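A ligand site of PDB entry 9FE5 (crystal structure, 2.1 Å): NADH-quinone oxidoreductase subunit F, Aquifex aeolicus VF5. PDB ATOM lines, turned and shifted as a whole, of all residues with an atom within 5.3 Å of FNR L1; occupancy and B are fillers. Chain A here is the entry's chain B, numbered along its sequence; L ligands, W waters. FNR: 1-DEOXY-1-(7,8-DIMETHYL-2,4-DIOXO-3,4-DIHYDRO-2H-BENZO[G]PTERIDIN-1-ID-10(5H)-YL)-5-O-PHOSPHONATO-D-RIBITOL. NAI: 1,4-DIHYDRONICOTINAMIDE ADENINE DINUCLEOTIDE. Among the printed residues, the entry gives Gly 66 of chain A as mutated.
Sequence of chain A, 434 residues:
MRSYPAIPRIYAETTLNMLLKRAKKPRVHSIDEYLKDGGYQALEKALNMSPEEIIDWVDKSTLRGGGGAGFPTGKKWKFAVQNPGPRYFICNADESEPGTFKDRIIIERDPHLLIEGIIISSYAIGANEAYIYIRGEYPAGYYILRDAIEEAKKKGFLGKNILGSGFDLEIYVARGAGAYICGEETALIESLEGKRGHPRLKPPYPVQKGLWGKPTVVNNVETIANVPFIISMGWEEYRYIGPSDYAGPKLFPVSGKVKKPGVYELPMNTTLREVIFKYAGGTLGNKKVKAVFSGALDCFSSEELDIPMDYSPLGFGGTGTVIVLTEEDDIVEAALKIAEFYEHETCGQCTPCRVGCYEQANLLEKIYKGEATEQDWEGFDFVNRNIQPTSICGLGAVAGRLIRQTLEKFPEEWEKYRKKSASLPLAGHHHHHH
N of Gly 66 lies within hydrogen-bond range of O2P of FNR L1, at 3.5 Å.
The backbone NH (N) of Asn 220 sits at hydrogen-bond distance from an oxygen (O3P) of FNR L1.
An oxygen (O2B) of NAI L2 lies within hydrogen-bond range of the side-chain carboxylate of Glu 185 (2.5 Å).
The backbone NH (N) of Glu 95 is in hydrogen-bond range of an oxygen (O4) of FNR L1, 3.0 Å away.
A nitrogen (N5) of FNR L1 sits close to the backbone carbonyl oxygen of Gly 183, 3.3 Å away.
The side-chain hydroxyl (OG1) of Thr 223 sits at hydrogen-bond distance from an oxygen (O3P) of FNR L1.
O of Gly 67 lies close to N7N of NAI L2 (3.5 Å).
The side-chain amide nitrogen of Asn 92 lies within hydrogen-bond range of an oxygen (O4') of FNR L1, at 3.1 Å.
N of Gly 67 sits at hydrogen-bond distance from O2P of FNR L1, at 2.8 Å.
N of Glu 185 is in hydrogen-bond range of O2' of FNR L1 (3.1 Å).
The backbone carbonyl oxygen (O) of Gly 67 lies within hydrogen-bond range of a nitrogen (N1) of FNR L1.
The side-chain amide oxygen of Asn 220 sits close to an oxygen (O2) of FNR L1, at 2.7 Å.
An oxygen (O3B) of NAI L2 lies within hydrogen-bond range of the side-chain amino group (NZ) of Lys 76, at 2.8 Å.
O2N of NAI L2 lies within salt-bridge range of NZ of Lys 202 (3.5 Å).
The backbone carbonyl oxygen (O) of Gly 68 lies within hydrogen-bond range of an oxygen (O3D) of NAI L2.
NZ of Lys 76 lies within salt-bridge range of O1P of FNR L1, at 2.6 Å.
The side-chain amide oxygen (OD1) of Asn 219 lies close to an oxygen (O3P) of FNR L1, 2.8 Å away.
An oxygen (O3') of FNR L1 sits at hydrogen-bond distance from an oxygen (O2N) of NAI L2, 2.7 Å away.
The backbone NH of Gly 70 sits close to the backbone carbonyl oxygen of Gly 65 (3.4 Å).
The backbone NH (N) of Asp 94 lies within hydrogen-bond range of the side-chain amide oxygen (OD1) of Asn 92 (3.1 Å).
The backbone carbonyl oxygen (O) of Gly 66 lies within hydrogen-bond range of the side-chain amide nitrogen (ND2) of Asn 220, at 3.3 Å.
The backbone NH (N) of Gly 65 sits at hydrogen-bond distance from the backbone carbonyl oxygen (O) of Phe 71.
The backbone carbonyl oxygen (O) of Asn 92 lies within hydrogen-bond range of the backbone NH (N) of Val 221 (3.4 Å).
OD2 of Asp 103 lies close to OD1 of Asn 220 (2.8 Å).
The side-chain amino group (NZ) of Lys 76 is in hydrogen-bond range of the backbone carbonyl oxygen (O) of Val 218 (2.8 Å).
The backbone NH (N) of Asp 103 lies within hydrogen-bond range of the side-chain carboxylate (OE2) of Glu 95 (2.7 Å).
The backbone carbonyl oxygen of Val 218 sits close to an oxygen (O5') of FNR L1.
CA of Gly 65 touches O2P of FNR L1 (3.3 Å).
C of Asp 94 touches O4 of FNR L1 (3.5 Å).
N of Ser 96 touches O4 of FNR L1 (3.8 Å).
Tyr 180 touches FNR L1 (CE2 to C7M, 3.6 Å).
Ile 181 touches FNR L1.
Glu 184 touches FNR L1 (N to C5A, 3.5 Å).
Gly 394 touches FNR L1 (N to C8M, 3.8 Å).
Leu 395 touches FNR L1 (CB to C7M, 3.9 Å).
Hydrophobic or aromatic side chains that line FNR L1: Tyr 180, Ile 181, Val 218 and Leu 395.
19 residues have an atom within 4 Å of FNR L1: Gly 65, Gly 66, Gly 67, Lys 76, Asn 92, Asp 94, Glu 95, Ser 96, Tyr 180, Ile 181, Gly 183, Glu 184, Glu 185, Val 218, Asn 219, Asn 220, Thr 223, Gly 394 and Leu 395.
The nearest printed residue that does not touch FNR L1 is Gly 68 (4.1 Å).
Water W2 lies within hydrogen-bond range of O2P of FNR L1 (2.6 Å), N of Ala 69 (2.9 Å) and N of Gly 68 (3.1 Å).
Water W1 lies within hydrogen-bond range of O1P of FNR L1, N of Phe 71 and N of Gly 70.
Water W5 lies within hydrogen-bond range of the backbone carbonyl oxygen (O) of Phe 71 (2.8 Å), the side-chain hydroxyl (OG1) of Thr 73 (2.8 Å), an oxygen (O1P) of FNR L1 (2.8 Å) and the side-chain amide oxygen (OD1) of Asn 219 (3.2 Å).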
ATOM      1  N   GLY A  65     -10.217 -22.668   0.497  1.00  0.00           N
ATOM      2  CA  GLY A  65      -9.758 -22.250   1.810  1.00  0.00           C
ATOM      3  C   GLY A  65      -8.706 -21.158   1.701  1.00  0.00           C
ATOM      4  O   GLY A  65      -7.813 -21.230   0.863  1.00  0.00           O
ATOM      5  N   GLY A  66      -8.828 -20.133   2.550  1.00  0.00           N
ATOM      6  CA  GLY A  66      -7.872 -19.039   2.592  1.00  0.00           C
ATOM      7  C   GLY A  66      -6.864 -19.205   3.715  1.00  0.00           C
ATOM      8  O   GLY A  66      -6.099 -18.292   4.013  1.00  0.00           O
ATOM      9  N   GLY A  67      -6.871 -20.401   4.336  1.00  0.00           N
ATOM     10  CA  GLY A  67      -5.964 -20.716   5.427  1.00  0.00           C
ATOM     11  C   GLY A  67      -4.618 -21.233   4.940  1.00  0.00           C
ATOM     12  O   GLY A  67      -3.732 -21.487   5.747  1.00  0.00           O
ATOM     13  N   GLY A  68      -4.475 -21.453   3.624  1.00  0.00           N
ATOM     14  CA  GLY A  68      -3.162 -21.715   3.038  1.00  0.00           C
ATOM     15  C   GLY A  68      -3.150 -22.892   2.069  1.00  0.00           C
ATOM     16  O   GLY A  68      -2.353 -22.907   1.133  1.00  0.00           O
ATOM     17  N   ALA A  69      -4.026 -23.882   2.272  1.00  0.00           N
ATOM     18  CA  ALA A  69      -4.014 -25.087   1.440  1.00  0.00           C
ATOM     19  C   ALA A  69      -4.973 -24.986   0.255  1.00  0.00           C
ATOM     20  O   ALA A  69      -4.910 -25.807  -0.655  1.00  0.00           O
ATOM     21  CB  ALA A  69      -4.323 -26.291   2.297  1.00  0.00           C
ATOM     22  N   GLY A  70      -5.891 -24.006   0.268  1.00  0.00           N
ATOM     23  CA  GLY A  70      -6.808 -23.780  -0.846  1.00  0.00           C
ATOM     24  C   GLY A  70      -7.722 -24.976  -1.119  1.00  0.00           C
ATOM     25  O   GLY A  70      -8.082 -25.219  -2.267  1.00  0.00           O
ATOM     26  N   PHE A  71      -8.121 -25.701  -0.075  1.00  0.00           N
ATOM     27  CA  PHE A  71      -8.993 -26.851  -0.263  1.00  0.00           C
ATOM     28  C   PHE A  71     -10.416 -26.379  -0.560  1.00  0.00           C
ATOM     29  O   PHE A  71     -10.908 -25.460   0.099  1.00  0.00           O
ATOM     30  CB  PHE A  71      -8.963 -27.795   0.947  1.00  0.00           C
ATOM     31  CG  PHE A  71      -9.641 -29.127   0.712  1.00  0.00           C
ATOM     32  CD1 PHE A  71      -8.949 -30.197   0.168  1.00  0.00           C
ATOM     33  CD2 PHE A  71     -10.990 -29.315   1.017  1.00  0.00           C
ATOM     34  CE1 PHE A  71      -9.573 -31.423  -0.066  1.00  0.00           C
ATOM     35  CE2 PHE A  71     -11.613 -30.533   0.800  1.00  0.00           C
ATOM     36  CZ  PHE A  71     -10.905 -31.587   0.259  1.00  0.00           C
ATOM     37  N   THR A  73     -14.063 -25.594  -0.256  1.00  0.00           N
ATOM     38  CA  THR A  73     -14.802 -25.482   0.986  1.00  0.00           C
ATOM     39  C   THR A  73     -16.056 -26.361   0.928  1.00  0.00           C
ATOM     40  O   THR A  73     -16.351 -27.083   1.885  1.00  0.00           O
ATOM     41  CB  THR A  73     -15.135 -24.023   1.229  1.00  0.00           C
ATOM     42  OG1 THR A  73     -13.905 -23.300   1.208  1.00  0.00           O
ATOM     43  CG2 THR A  73     -15.884 -23.822   2.540  1.00  0.00           C
ATOM     44  N   LYS A  76     -15.373 -29.943   1.429  1.00  0.00           N
ATOM     45  CA  LYS A  76     -15.077 -30.176   2.833  1.00  0.00           C
ATOM     46  C   LYS A  76     -16.374 -30.372   3.617  1.00  0.00           C
ATOM     47  O   LYS A  76     -16.511 -31.326   4.386  1.00  0.00           O
ATOM     48  CB  LYS A  76     -14.260 -29.023   3.423  1.00  0.00           C
ATOM     49  CG  LYS A  76     -13.639 -29.334   4.776  1.00  0.00           C
ATOM     50  CD  LYS A  76     -12.912 -28.177   5.470  1.00  0.00           C
ATOM     51  CE  LYS A  76     -11.689 -27.670   4.776  1.00  0.00           C
ATOM     52  NZ  LYS A  76     -10.954 -26.756   5.653  1.00  0.00           N
ATOM     53  N   ASN A  92     -10.957 -20.714  12.306  1.00  0.00           N
ATOM     54  CA  ASN A  92      -9.539 -20.663  12.608  1.00  0.00           C
ATOM     55  C   ASN A  92      -9.030 -19.233  12.462  1.00  0.00           C
ATOM     56  O   ASN A  92      -8.799 -18.762  11.352  1.00  0.00           O
ATOM     57  CB  ASN A  92      -8.734 -21.605  11.716  1.00  0.00           C
ATOM     58  CG  ASN A  92      -7.325 -21.825  12.205  1.00  0.00           C
ATOM     59  OD1 ASN A  92      -6.744 -20.991  12.920  1.00  0.00           O
ATOM     60  ND2 ASN A  92      -6.725 -22.920  11.769  1.00  0.00           N
ATOM     61  N   ASP A  94      -6.143 -18.208  14.140  1.00  0.00           N
ATOM     62  CA  ASP A  94      -4.860 -18.306  14.823  1.00  0.00           C
ATOM     63  C   ASP A  94      -3.777 -17.495  14.113  1.00  0.00           C
ATOM     64  O   ASP A  94      -2.767 -17.185  14.740  1.00  0.00           O
ATOM     65  CB  ASP A  94      -4.365 -19.726  15.029  1.00  0.00           C
ATOM     66  CG  ASP A  94      -3.285 -19.804  16.104  1.00  0.00           C
ATOM     67  OD1 ASP A  94      -3.624 -19.526  17.273  1.00  0.00           O
ATOM     68  OD2 ASP A  94      -2.107 -20.037  15.747  1.00  0.00           O
ATOM     69  N   GLU A  95      -4.004 -17.160  12.833  1.00  0.00           N
ATOM     70  CA  GLU A  95      -3.115 -16.350  12.004  1.00  0.00           C
ATOM     71  C   GLU A  95      -1.806 -15.981  12.694  1.00  0.00           C
ATOM     72  O   GLU A  95      -1.695 -14.915  13.296  1.00  0.00           O
ATOM     73  CB  GLU A  95      -3.856 -15.070  11.594  1.00  0.00           C
ATOM     74  CG  GLU A  95      -3.050 -14.211  10.624  1.00  0.00           C
ATOM     75  CD  GLU A  95      -3.889 -13.148   9.947  1.00  0.00           C
ATOM     76  OE1 GLU A  95      -4.276 -12.183  10.654  1.00  0.00           O
ATOM     77  OE2 GLU A  95      -4.147 -13.280   8.738  1.00  0.00           O
ATOM     78  N   SER A  96      -0.779 -16.837  12.536  1.00  0.00           N
ATOM     79  CA  SER A  96       0.524 -16.578  13.112  1.00  0.00           C
ATOM     80  C   SER A  96       1.704 -16.806  12.151  1.00  0.00           C
ATOM     81  O   SER A  96       2.853 -16.703  12.590  1.00  0.00           O
ATOM     82  CB  SER A  96       0.696 -17.382  14.377  1.00  0.00           C
ATOM     83  OG  SER A  96      -0.182 -16.911  15.389  1.00  0.00           O
ATOM     84  N   ASP A 103      -6.355 -11.794   8.173  1.00  0.00           N
ATOM     85  CA  ASP A 103      -7.575 -12.196   8.872  1.00  0.00           C
ATOM     86  C   ASP A 103      -7.958 -11.187   9.947  1.00  0.00           C
ATOM     87  O   ASP A 103      -9.145 -10.957  10.183  1.00  0.00           O
ATOM     88  CB  ASP A 103      -7.438 -13.580   9.474  1.00  0.00           C
ATOM     89  CG  ASP A 103      -7.201 -14.712   8.491  1.00  0.00           C
ATOM     90  OD1 ASP A 103      -7.491 -14.518   7.283  1.00  0.00           O
ATOM     91  OD2 ASP A 103      -6.694 -15.767   8.931  1.00  0.00           O
ATOM     92  N   TYR A 180       2.296 -21.206  17.445  1.00  0.00           N
ATOM     93  CA  TYR A 180       1.952 -21.161  16.035  1.00  0.00           C
ATOM     94  C   TYR A 180       1.287 -22.459  15.582  1.00  0.00           C
ATOM     95  O   TYR A 180       0.459 -22.460  14.683  1.00  0.00           O
ATOM     96  CB  TYR A 180       3.220 -20.897  15.209  1.00  0.00           C
ATOM     97  CG  TYR A 180       3.164 -21.228  13.727  1.00  0.00           C
ATOM     98  CD1 TYR A 180       2.495 -20.416  12.825  1.00  0.00           C
ATOM     99  CD2 TYR A 180       3.846 -22.337  13.214  1.00  0.00           C
ATOM    100  CE1 TYR A 180       2.468 -20.695  11.471  1.00  0.00           C
ATOM    101  CE2 TYR A 180       3.840 -22.625  11.863  1.00  0.00           C
ATOM    102  CZ  TYR A 180       3.136 -21.807  10.983  1.00  0.00           C
ATOM    103  OH  TYR A 180       3.130 -22.099   9.656  1.00  0.00           O
ATOM    104  N   ILE A 181       1.693 -23.574  16.203  1.00  0.00           N
ATOM    105  CA  ILE A 181       1.248 -24.887  15.776  1.00  0.00           C
ATOM    106  C   ILE A 181      -0.262 -25.040  16.008  1.00  0.00           C
ATOM    107  O   ILE A 181      -0.903 -25.848  15.351  1.00  0.00           O
ATOM    108  CB  ILE A 181       2.061 -25.996  16.467  1.00  0.00           C
ATOM    109  CG1 ILE A 181       1.871 -27.340  15.781  1.00  0.00           C
ATOM    110  CG2 ILE A 181       1.720 -26.084  17.956  1.00  0.00           C
ATOM    111  CD1 ILE A 181       2.211 -27.336  14.299  1.00  0.00           C
ATOM    112  N   GLY A 183      -2.462 -23.243  15.048  1.00  0.00           N
ATOM    113  CA  GLY A 183      -3.157 -22.908  13.810  1.00  0.00           C
ATOM    114  C   GLY A 183      -3.382 -24.135  12.938  1.00  0.00           C
ATOM    115  O   GLY A 183      -4.273 -24.131  12.085  1.00  0.00           O
ATOM    116  N   GLU A 184      -2.551 -25.177  13.139  1.00  0.00           N
ATOM    117  CA  GLU A 184      -2.778 -26.473  12.511  1.00  0.00           C
ATOM    118  C   GLU A 184      -4.081 -27.033  13.081  1.00  0.00           C
ATOM    119  O   GLU A 184      -4.251 -27.064  14.297  1.00  0.00           O
ATOM    120  CB  GLU A 184      -1.595 -27.409  12.737  1.00  0.00           C
ATOM    121  CG  GLU A 184      -1.533 -28.584  11.764  1.00  0.00           C
ATOM    122  CD  GLU A 184      -2.434 -29.770  12.063  1.00  0.00           C
ATOM    123  OE1 GLU A 184      -2.902 -29.917  13.211  1.00  0.00           O
ATOM    124  OE2 GLU A 184      -2.647 -30.574  11.119  1.00  0.00           O
ATOM    125  N   GLU A 185      -4.987 -27.466  12.205  1.00  0.00           N
ATOM    126  CA  GLU A 185      -6.375 -27.702  12.581  1.00  0.00           C
ATOM    127  C   GLU A 185      -6.513 -28.742  13.692  1.00  0.00           C
ATOM    128  O   GLU A 185      -7.352 -28.560  14.573  1.00  0.00           O
ATOM    129  CB  GLU A 185      -7.222 -28.042  11.357  1.00  0.00           C
ATOM    130  CG  GLU A 185      -6.871 -29.379  10.720  1.00  0.00           C
ATOM    131  CD  GLU A 185      -7.651 -29.672   9.458  1.00  0.00           C
ATOM    132  OE1 GLU A 185      -8.604 -28.912   9.156  1.00  0.00           O
ATOM    133  OE2 GLU A 185      -7.295 -30.675   8.794  1.00  0.00           O
ATOM    134  N   LYS A 202      -3.279 -37.413  10.432  1.00  0.00           N
ATOM    135  CA  LYS A 202      -4.368 -37.312   9.468  1.00  0.00           C
ATOM    136  C   LYS A 202      -4.056 -38.210   8.267  1.00  0.00           C
ATOM    137  O   LYS A 202      -2.913 -38.209   7.799  1.00  0.00           O
ATOM    138  CB  LYS A 202      -4.529 -35.890   8.938  1.00  0.00           C
ATOM    139  CG  LYS A 202      -4.864 -34.826   9.972  1.00  0.00           C
ATOM    140  CD  LYS A 202      -4.312 -33.435   9.642  1.00  0.00           C
ATOM    141  CE  LYS A 202      -4.876 -32.787   8.423  1.00  0.00           C
ATOM    142  NZ  LYS A 202      -4.562 -31.344   8.396  1.00  0.00           N
ATOM    143  N   VAL A 218     -13.203 -27.258  10.163  1.00  0.00           N
ATOM    144  CA  VAL A 218     -12.351 -26.120  10.468  1.00  0.00           C
ATOM    145  C   VAL A 218     -12.182 -25.308   9.187  1.00  0.00           C
ATOM    146  O   VAL A 218     -11.788 -25.856   8.168  1.00  0.00           O
ATOM    147  CB  VAL A 218     -10.984 -26.568  11.014  1.00  0.00           C
ATOM    148  CG1 VAL A 218     -10.125 -25.382  11.452  1.00  0.00           C
ATOM    149  CG2 VAL A 218     -11.140 -27.570  12.152  1.00  0.00           C
ATOM    150  N   ASN A 219     -12.527 -24.006   9.251  1.00  0.00           N
ATOM    151  CA  ASN A 219     -12.271 -23.076   8.162  1.00  0.00           C
ATOM    152  C   ASN A 219     -11.601 -21.810   8.697  1.00  0.00           C
ATOM    153  O   ASN A 219     -11.857 -21.400   9.829  1.00  0.00           O
ATOM    154  CB  ASN A 219     -13.541 -22.685   7.404  1.00  0.00           C
ATOM    155  CG  ASN A 219     -13.882 -23.669   6.311  1.00  0.00           C
ATOM    156  OD1 ASN A 219     -13.078 -23.908   5.404  1.00  0.00           O
ATOM    157  ND2 ASN A 219     -15.042 -24.283   6.408  1.00  0.00           N
ATOM    158  N   ASN A 220     -10.784 -21.210   7.829  1.00  0.00           N
ATOM    159  CA  ASN A 220     -10.092 -19.954   8.088  1.00  0.00           C
ATOM    160  C   ASN A 220     -11.078 -18.787   8.049  1.00  0.00           C
ATOM    161  O   ASN A 220     -12.100 -18.845   7.369  1.00  0.00           O
ATOM    162  CB  ASN A 220      -8.949 -19.835   7.086  1.00  0.00           C
ATOM    163  CG  ASN A 220      -8.226 -18.516   7.157  1.00  0.00           C
ATOM    164  OD1 ASN A 220      -7.377 -18.307   8.033  1.00  0.00           O
ATOM    165  ND2 ASN A 220      -8.513 -17.641   6.210  1.00  0.00           N
ATOM    166  N   VAL A 221     -10.749 -17.707   8.786  1.00  0.00           N
ATOM    167  CA  VAL A 221     -11.521 -16.473   8.844  1.00  0.00           C
ATOM    168  C   VAL A 221     -11.936 -16.009   7.436  1.00  0.00           C
ATOM    169  O   VAL A 221     -13.119 -15.772   7.203  1.00  0.00           O
ATOM    170  CB  VAL A 221     -10.722 -15.380   9.564  1.00  0.00           C
ATOM    171  CG1 VAL A 221     -11.326 -13.985   9.367  1.00  0.00           C
ATOM    172  CG2 VAL A 221     -10.566 -15.682  11.045  1.00  0.00           C
ATOM    173  N   THR A 223     -12.035 -17.555   4.541  1.00  0.00           N
ATOM    174  CA  THR A 223     -12.952 -18.504   3.915  1.00  0.00           C
ATOM    175  C   THR A 223     -14.384 -18.192   4.340  1.00  0.00           C
ATOM    176  O   THR A 223     -15.277 -18.072   3.498  1.00  0.00           O
ATOM    177  CB  THR A 223     -12.584 -19.944   4.283  1.00  0.00           C
ATOM    178  OG1 THR A 223     -11.194 -20.135   4.036  1.00  0.00           O
ATOM    179  CG2 THR A 223     -13.384 -20.967   3.496  1.00  0.00           C
ATOM    180  N   CYS A 393       2.573 -33.498  10.538  1.00  0.00           N
ATOM    181  CA  CYS A 393       1.861 -32.284  10.113  1.00  0.00           C
ATOM    182  C   CYS A 393       2.746 -31.484   9.166  1.00  0.00           C
ATOM    183  O   CYS A 393       3.902 -31.828   8.964  1.00  0.00           O
ATOM    184  CB  CYS A 393       1.386 -31.443  11.296  1.00  0.00           C
ATOM    185  SG  CYS A 393       2.574 -30.187  11.856  1.00  0.00           S
ATOM    186  N   GLY A 394       2.167 -30.402   8.607  1.00  0.00           N
ATOM    187  CA  GLY A 394       2.790 -29.646   7.521  1.00  0.00           C
ATOM    188  C   GLY A 394       4.016 -28.845   7.964  1.00  0.00           C
ATOM    189  O   GLY A 394       4.855 -28.523   7.129  1.00  0.00           O
ATOM    190  N   LEU A 395       4.127 -28.487   9.252  1.00  0.00           N
ATOM    191  CA  LEU A 395       5.279 -27.726   9.730  1.00  0.00           C
ATOM    192  C   LEU A 395       6.560 -28.504   9.439  1.00  0.00           C
ATOM    193  O   LEU A 395       7.475 -27.971   8.808  1.00  0.00           O
ATOM    194  CB  LEU A 395       5.150 -27.393  11.213  1.00  0.00           C
ATOM    195  CG  LEU A 395       6.164 -26.393  11.785  1.00  0.00           C
ATOM    196  CD1 LEU A 395       5.599 -25.755  13.051  1.00  0.00           C
ATOM    197  CD2 LEU A 395       7.522 -27.019  12.094  1.00  0.00           C
HETATM  198  C9A FNR L   1      -2.036 -24.191   9.448  1.00  0.00           C
HETATM  199  N10 FNR L   1      -3.295 -23.741   8.939  1.00  0.00           N
HETATM  200  CAA FNR L   1      -3.790 -22.513   9.359  1.00  0.00           C
HETATM  201  N1  FNR L   1      -5.017 -22.107   8.880  1.00  0.00           N
HETATM  202  C2  FNR L   1      -5.641 -20.971   9.332  1.00  0.00           C
HETATM  203  O2  FNR L   1      -6.800 -20.701   9.025  1.00  0.00           O
HETATM  204  N3  FNR L   1      -4.920 -20.179  10.180  1.00  0.00           N
HETATM  205  C4  FNR L   1      -3.672 -20.468  10.724  1.00  0.00           C
HETATM  206  O4  FNR L   1      -3.151 -19.675  11.507  1.00  0.00           O
HETATM  207  C4A FNR L   1      -3.124 -21.720  10.266  1.00  0.00           C
HETATM  208  N5  FNR L   1      -1.942 -22.163  10.789  1.00  0.00           N
HETATM  209  C5A FNR L   1      -1.382 -23.379  10.391  1.00  0.00           C
HETATM  210  C6  FNR L   1      -0.169 -23.795  10.942  1.00  0.00           C
HETATM  211  C7  FNR L   1       0.414 -25.002  10.550  1.00  0.00           C
HETATM  212  C7M FNR L   1       1.735 -25.413  11.148  1.00  0.00           C
HETATM  213  C8  FNR L   1      -0.240 -25.805   9.592  1.00  0.00           C
HETATM  214  C8M FNR L   1       0.382 -27.096   9.115  1.00  0.00           C
HETATM  215  C9  FNR L   1      -1.454 -25.397   9.055  1.00  0.00           C
HETATM  216  C1' FNR L   1      -4.073 -24.581   8.029  1.00  0.00           C
HETATM  217  C2' FNR L   1      -5.104 -25.387   8.809  1.00  0.00           C
HETATM  218  O2' FNR L   1      -4.488 -26.578   9.297  1.00  0.00           O
HETATM  219  C3' FNR L   1      -6.306 -25.715   7.915  1.00  0.00           C
HETATM  220  O3' FNR L   1      -5.860 -26.192   6.647  1.00  0.00           O
HETATM  221  C4' FNR L   1      -7.267 -24.544   7.694  1.00  0.00           C
HETATM  222  O4' FNR L   1      -7.572 -23.856   8.919  1.00  0.00           O
HETATM  223  C5' FNR L   1      -8.542 -25.002   7.023  1.00  0.00           C
HETATM  224  O5' FNR L   1      -9.351 -23.856   6.682  1.00  0.00           O
HETATM  225  P   FNR L   1      -9.528 -23.463   5.126  1.00  0.00           P
HETATM  226  O1P FNR L   1      -9.867 -24.720   4.364  1.00  0.00           O
HETATM  227  O2P FNR L   1      -8.231 -22.833   4.634  1.00  0.00           O
HETATM  228  O3P FNR L   1     -10.671 -22.468   5.191  1.00  0.00           O
HETATM  229  PA  NAI L   2      -4.112 -29.938   4.017  1.00  0.00           P
HETATM  230  O1A NAI L   2      -3.907 -29.948   2.562  1.00  0.00           O
HETATM  231  O2A NAI L   2      -3.744 -31.230   4.704  1.00  0.00           O
HETATM  232  O5B NAI L   2      -5.644 -29.695   4.394  1.00  0.00           O
HETATM  233  C5B NAI L   2      -6.331 -28.471   4.074  1.00  0.00           C
HETATM  234  C4B NAI L   2      -7.745 -28.562   4.581  1.00  0.00           C
HETATM  235  O4B NAI L   2      -8.499 -29.476   3.749  1.00  0.00           O
HETATM  236  C3B NAI L   2      -7.882 -29.084   6.009  1.00  0.00           C
HETATM  237  O3B NAI L   2      -8.990 -28.495   6.657  1.00  0.00           O
HETATM  238  C2B NAI L   2      -8.093 -30.587   5.803  1.00  0.00           C
HETATM  239  O2B NAI L   2      -8.819 -31.177   6.870  1.00  0.00           O
HETATM  240  C1B NAI L   2      -8.936 -30.589   4.527  1.00  0.00           C
HETATM  241  N9A NAI L   2      -8.795 -31.802   3.733  1.00  0.00           N
HETATM  242  C8A NAI L   2      -7.779 -32.128   2.865  1.00  0.00           C
HETATM  243  N7A NAI L   2      -7.922 -33.299   2.282  1.00  0.00           N
HETATM  244  C5A NAI L   2      -9.118 -33.780   2.807  1.00  0.00           C
HETATM  245  C6A NAI L   2      -9.852 -34.961   2.581  1.00  0.00           C
HETATM  246  N6A NAI L   2      -9.460 -35.921   1.738  1.00  0.00           N
HETATM  247  N1A NAI L   2     -10.999 -35.132   3.264  1.00  0.00           N
HETATM  248  C2A NAI L   2     -11.384 -34.175   4.119  1.00  0.00           C
HETATM  249  N3A NAI L   2     -10.793 -33.014   4.409  1.00  0.00           N
HETATM  250  C4A NAI L   2      -9.663 -32.867   3.705  1.00  0.00           C
HETATM  251  O3  NAI L   2      -3.296 -28.738   4.685  1.00  0.00           O
HETATM  252  PN  NAI L   2      -2.887 -28.283   6.162  1.00  0.00           P
HETATM  253  O1N NAI L   2      -1.902 -29.339   6.670  1.00  0.00           O
HETATM  254  O2N NAI L   2      -4.070 -28.136   7.039  1.00  0.00           O
HETATM  255  O5D NAI L   2      -2.129 -26.842   5.971  1.00  0.00           O
HETATM  256  C5D NAI L   2      -0.823 -26.472   5.449  1.00  0.00           C
HETATM  257  C4D NAI L   2      -0.879 -25.025   5.022  1.00  0.00           C
HETATM  258  O4D NAI L   2      -1.032 -24.150   6.157  1.00  0.00           O
HETATM  259  C3D NAI L   2       0.333 -24.476   4.252  1.00  0.00           C
HETATM  260  O3D NAI L   2       0.011 -24.426   2.871  1.00  0.00           O
HETATM  261  C2D NAI L   2       0.535 -23.056   4.822  1.00  0.00           C
HETATM  262  O2D NAI L   2       0.545 -22.045   3.822  1.00  0.00           O
HETATM  263  C1D NAI L   2      -0.714 -22.859   5.691  1.00  0.00           C
HETATM  264  N1N NAI L   2      -0.557 -21.940   6.827  1.00  0.00           N
HETATM  265  C2N NAI L   2      -1.345 -20.679   6.952  1.00  0.00           C
HETATM  266  C3N NAI L   2      -1.301 -19.882   8.044  1.00  0.00           C
HETATM  267  C7N NAI L   2      -2.140 -18.635   8.212  1.00  0.00           C
HETATM  268  O7N NAI L   2      -1.822 -17.757   9.035  1.00  0.00           O
HETATM  269  N7N NAI L   2      -3.244 -18.514   7.495  1.00  0.00           N
HETATM  270  C4N NAI L   2      -0.399 -20.252   9.151  1.00  0.00           C
HETATM  271  C5N NAI L   2       0.474 -21.418   8.863  1.00  0.00           C
HETATM  272  C6N NAI L   2       0.361 -22.195   7.800  1.00  0.00           C
HETATM  273  O   HOH W   1      -7.860 -25.434   2.770  1.00  0.00           O
HETATM  274  O   HOH W   2      -5.910 -24.039   4.467  1.00  0.00           O
HETATM  275  O   HOH W   3      -0.838 -20.335  13.169  1.00  0.00           O
HETATM  276  O   HOH W   4      -6.415 -17.714  10.896  1.00  0.00           O
HETATM  277  O   HOH W   5     -12.052 -24.880   2.566  1.00  0.00           O
